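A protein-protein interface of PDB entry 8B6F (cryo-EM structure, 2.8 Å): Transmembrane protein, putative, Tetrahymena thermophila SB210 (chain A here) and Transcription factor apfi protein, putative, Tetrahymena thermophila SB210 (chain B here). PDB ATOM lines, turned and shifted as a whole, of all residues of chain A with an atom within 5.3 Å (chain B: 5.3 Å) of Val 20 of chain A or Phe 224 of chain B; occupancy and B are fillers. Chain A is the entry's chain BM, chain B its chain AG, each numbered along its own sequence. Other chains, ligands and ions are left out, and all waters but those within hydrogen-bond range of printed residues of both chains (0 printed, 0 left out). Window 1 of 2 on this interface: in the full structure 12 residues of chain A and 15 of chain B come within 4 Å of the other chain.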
ATOM      1  N   ARG A  18       6.362 -14.375  -1.741  1.00  0.00           N
ATOM      2  CA  ARG A  18       5.486 -13.220  -1.606  1.00  0.00           C
ATOM      3  C   ARG A  18       4.047 -13.676  -1.419  1.00  0.00           C
ATOM      4  O   ARG A  18       3.575 -14.591  -2.098  1.00  0.00           O
ATOM      5  CB  ARG A  18       5.597 -12.328  -2.843  1.00  0.00           C
ATOM      6  CG  ARG A  18       4.872 -10.997  -2.725  1.00  0.00           C
ATOM      7  CD  ARG A  18       5.643 -10.026  -1.852  1.00  0.00           C
ATOM      8  NE  ARG A  18       4.944  -8.756  -1.696  1.00  0.00           N
ATOM      9  CZ  ARG A  18       4.103  -8.472  -0.711  1.00  0.00           C
ATOM     10  NH1 ARG A  18       3.820  -9.352   0.234  1.00  0.00           N
ATOM     11  NH2 ARG A  18       3.533  -7.271  -0.670  1.00  0.00           N
ATOM     12  N   ARG A  19       3.345 -13.035  -0.487  1.00  0.00           N
ATOM     13  CA  ARG A  19       1.975 -13.430  -0.190  1.00  0.00           C
ATOM     14  C   ARG A  19       1.269 -12.311   0.558  1.00  0.00           C
ATOM     15  O   ARG A  19       1.768 -11.836   1.580  1.00  0.00           O
ATOM     16  CB  ARG A  19       1.953 -14.722   0.634  1.00  0.00           C
ATOM     17  CG  ARG A  19       0.572 -15.113   1.129  1.00  0.00           C
ATOM     18  CD  ARG A  19       0.558 -16.525   1.690  1.00  0.00           C
ATOM     19  NE  ARG A  19      -0.746 -16.873   2.239  1.00  0.00           N
ATOM     20  CZ  ARG A  19      -1.807 -17.194   1.511  1.00  0.00           C
ATOM     21  NH1 ARG A  19      -1.760 -17.210   0.189  1.00  0.00           N
ATOM     22  NH2 ARG A  19      -2.946 -17.502   2.124  1.00  0.00           N
ATOM     23  N   VAL A  20       0.114 -11.898   0.042  1.00  0.00           N
ATOM     24  CA  VAL A  20      -0.775 -10.965   0.723  1.00  0.00           C
ATOM     25  C   VAL A  20      -2.142 -11.628   0.807  1.00  0.00           C
ATOM     26  O   VAL A  20      -2.733 -11.966  -0.224  1.00  0.00           O
ATOM     27  CB  VAL A  20      -0.869  -9.612  -0.001  1.00  0.00           C
ATOM     28  CG1 VAL A  20      -1.749  -8.648   0.780  1.00  0.00           C
ATOM     29  CG2 VAL A  20       0.512  -9.023  -0.212  1.00  0.00           C
ATOM     30  N   VAL A  21      -2.644 -11.813   2.027  1.00  0.00           N
ATOM     31  CA  VAL A  21      -3.892 -12.538   2.220  1.00  0.00           C
ATOM     32  C   VAL A  21      -5.062 -11.688   1.748  1.00  0.00           C
ATOM     33  O   VAL A  21      -5.115 -10.474   1.989  1.00  0.00           O
ATOM     34  CB  VAL A  21      -4.055 -12.944   3.694  1.00  0.00           C
ATOM     35  CG1 VAL A  21      -5.428 -13.555   3.944  1.00  0.00           C
ATOM     36  CG2 VAL A  21      -2.966 -13.919   4.089  1.00  0.00           C
ATOM     37  N   ASP A  22      -6.013 -12.329   1.074  1.00  0.00           N
ATOM     38  CA  ASP A  22      -7.190 -11.643   0.553  1.00  0.00           C
ATOM     39  C   ASP A  22      -8.143 -11.331   1.700  1.00  0.00           C
ATOM     40  O   ASP A  22      -8.766 -12.236   2.265  1.00  0.00           O
ATOM     41  CB  ASP A  22      -7.869 -12.510  -0.504  1.00  0.00           C
ATOM     42  CG  ASP A  22      -8.985 -11.787  -1.221  1.00  0.00           C
ATOM     43  OD1 ASP A  22      -9.142 -10.569  -1.006  1.00  0.00           O
ATOM     44  OD2 ASP A  22      -9.708 -12.441  -2.002  1.00  0.00           O
ATOM     45  N   LYS B 222      -3.454   6.105   2.060  1.00  0.00           N
ATOM     46  CA  LYS B 222      -4.342   4.957   2.153  1.00  0.00           C
ATOM     47  C   LYS B 222      -3.532   3.676   2.039  1.00  0.00           C
ATOM     48  O   LYS B 222      -2.519   3.621   1.337  1.00  0.00           O
ATOM     49  CB  LYS B 222      -5.423   4.981   1.063  1.00  0.00           C
ATOM     50  CG  LYS B 222      -6.576   5.925   1.353  1.00  0.00           C
ATOM     51  CD  LYS B 222      -7.656   5.816   0.288  1.00  0.00           C
ATOM     52  CE  LYS B 222      -8.843   6.711   0.613  1.00  0.00           C
ATOM     53  NZ  LYS B 222      -9.904   6.629  -0.429  1.00  0.00           N
ATOM     54  N   SER B 223      -3.989   2.643   2.739  1.00  0.00           N
ATOM     55  CA  SER B 223      -3.341   1.345   2.672  1.00  0.00           C
ATOM     56  C   SER B 223      -3.670   0.658   1.349  1.00  0.00           C
ATOM     57  O   SER B 223      -4.588   1.046   0.623  1.00  0.00           O
ATOM     58  CB  SER B 223      -3.783   0.470   3.843  1.00  0.00           C
ATOM     59  OG  SER B 223      -3.228  -0.830   3.745  1.00  0.00           O
ATOM     60  N   PHE B 224      -2.904  -0.389   1.038  1.00  0.00           N
ATOM     61  CA  PHE B 224      -3.173  -1.150  -0.176  1.00  0.00           C
ATOM     62  C   PHE B 224      -4.566  -1.762  -0.142  1.00  0.00           C
ATOM     63  O   PHE B 224      -5.286  -1.744  -1.147  1.00  0.00           O
ATOM     64  CB  PHE B 224      -2.111  -2.231  -0.373  1.00  0.00           C
ATOM     65  CG  PHE B 224      -2.588  -3.401  -1.179  1.00  0.00           C
ATOM     66  CD1 PHE B 224      -3.064  -3.231  -2.469  1.00  0.00           C
ATOM     67  CD2 PHE B 224      -2.530  -4.681  -0.659  1.00  0.00           C
ATOM     68  CE1 PHE B 224      -3.504  -4.313  -3.207  1.00  0.00           C
ATOM     69  CE2 PHE B 224      -2.964  -5.763  -1.395  1.00  0.00           C
ATOM     70  CZ  PHE B 224      -3.447  -5.578  -2.674  1.00  0.00           C
ATOM     71  N   ARG B 225      -4.965  -2.309   1.006  1.00  0.00           N
ATOM     72  CA  ARG B 225      -6.299  -2.888   1.116  1.00  0.00           C
ATOM     73  C   ARG B 225      -7.374  -1.829   0.919  1.00  0.00           C
ATOM     74  O   ARG B 225      -8.396  -2.084   0.271  1.00  0.00           O
ATOM     75  CB  ARG B 225      -6.457  -3.575   2.472  1.00  0.00           C
ATOM     76  CG  ARG B 225      -5.421  -4.658   2.730  1.00  0.00           C
ATOM     77  CD  ARG B 225      -5.750  -5.453   3.984  1.00  0.00           C
ATOM     78  NE  ARG B 225      -4.719  -6.438   4.290  1.00  0.00           N
ATOM     79  CZ  ARG B 225      -4.634  -7.637   3.730  1.00  0.00           C
ATOM     80  NH1 ARG B 225      -5.496  -8.032   2.811  1.00  0.00           N
ATOM     81  NH2 ARG B 225      -3.655  -8.457   4.099  1.00  0.00           N
ATOM     82  N   GLU B 226      -7.167  -0.634   1.473  1.00  0.00           N
ATOM     83  CA  GLU B 226      -8.148   0.433   1.306  1.00  0.00           C
ATOM     84  C   GLU B 226      -8.233   0.888  -0.147  1.00  0.00           C
ATOM     85  O   GLU B 226      -9.325   1.170  -0.650  1.00  0.00           O
ATOM     86  CB  GLU B 226      -7.800   1.604   2.221  1.00  0.00           C
ATOM     87  CG  GLU B 226      -8.912   2.626   2.356  1.00  0.00           C
ATOM     88  CD  GLU B 226      -8.662   3.608   3.485  1.00  0.00           C
ATOM     89  OE1 GLU B 226      -7.595   3.517   4.126  1.00  0.00           O
ATOM     90  OE2 GLU B 226      -9.535   4.466   3.733  1.00  0.00           O
ATOM     91  N   VAL B 227      -7.094   0.966  -0.838  1.00  0.00           N
ATOM     92  CA  VAL B 227      -7.110   1.332  -2.252  1.00  0.00           C
ATOM     93  C   VAL B 227      -7.830   0.265  -3.062  1.00  0.00           C
ATOM     94  O   VAL B 227      -8.611   0.573  -3.970  1.00  0.00           O
ATOM     95  CB  VAL B 227      -5.677   1.564  -2.766  1.00  0.00           C
ATOM     96  CG1 VAL B 227      -5.672   1.770  -4.275  1.00  0.00           C
ATOM     97  CG2 VAL B 227      -5.052   2.761  -2.074  1.00  0.00           C
ATOM     98  N   LEU B 228      -7.584  -1.005  -2.744  1.00  0.00           N
ATOM     99  CA  LEU B 228      -8.286  -2.087  -3.425  1.00  0.00           C
ATOM    100  C   LEU B 228      -9.786  -1.995  -3.179  1.00  0.00           C
ATOM    101  O   LEU B 228     -10.588  -2.214  -4.094  1.00  0.00           O
ATOM    102  CB  LEU B 228      -7.743  -3.436  -2.958  1.00  0.00           C
ATOM    103  CG  LEU B 228      -8.206  -4.660  -3.751  1.00  0.00           C
ATOM    104  CD1 LEU B 228      -7.648  -4.634  -5.166  1.00  0.00           C
ATOM    105  CD2 LEU B 228      -7.799  -5.938  -3.043  1.00  0.00           C
ATOM    106  N   ASN B 229     -10.182  -1.675  -1.947  1.00  0.00           N
ATOM    107  CA  ASN B 229     -11.599  -1.496  -1.648  1.00  0.00           C
ATOM    108  C   ASN B 229     -12.184  -0.333  -2.437  1.00  0.00           C
ATOM    109  O   ASN B 229     -13.327  -0.404  -2.903  1.00  0.00           O
ATOM    110  CB  ASN B 229     -11.794  -1.280  -0.147  1.00  0.00           C
ATOM    111  CG  ASN B 229     -11.504  -2.527   0.660  1.00  0.00           C
ATOM    112  OD1 ASN B 229     -11.610  -3.644   0.155  1.00  0.00           O
ATOM    113  ND2 ASN B 229     -11.138  -2.342   1.923  1.00  0.00           N
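The guanidinium group (NH1) of Arg 225 of chain B is in hydrogen-bond range of the backbone carbonyl oxygen (O) of Val 21 of chain A.
The side-chain amide nitrogen (ND2) of Asn 229 of chain B sits close to the backbone carbonyl oxygen (O) of Arg 225 of chain B (3.2 Å).
Among the printed residues, pairs that only touch across the chains: Val 20 of chain A with Phe 224 of chain B (3.8 Å) and Val 20 of chain A with Arg 225 of chain B (3.8 Å).
Of chain B, only Phe 224 and Arg 225 come within 4 Å of Val 20 of chain A.
Phe 224 of chain B touches just one residue of chain A: Val 20 (3.8 Å).
Of the printed residues of chain A, Arg 225 of chain B touches Val 20 (3.8 Å) and Val 21 (2.6 Å).
Printed residues of chain B within 4 Å of Val 21 of chain A: Arg 225.
The nearest printed residue of chain B that does not touch Val 20 of chain A is Leu 228 of chain B (7.7 Å).
The nearest printed residue of chain A that does not touch Phe 224 of chain B is Val 21 of chain A (6.2 Å).
Hydrophobic or aromatic side chains of chain A that line the printed part of chain B: Val 20.
Among the printed residues, 3 pairs touch across the chains.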
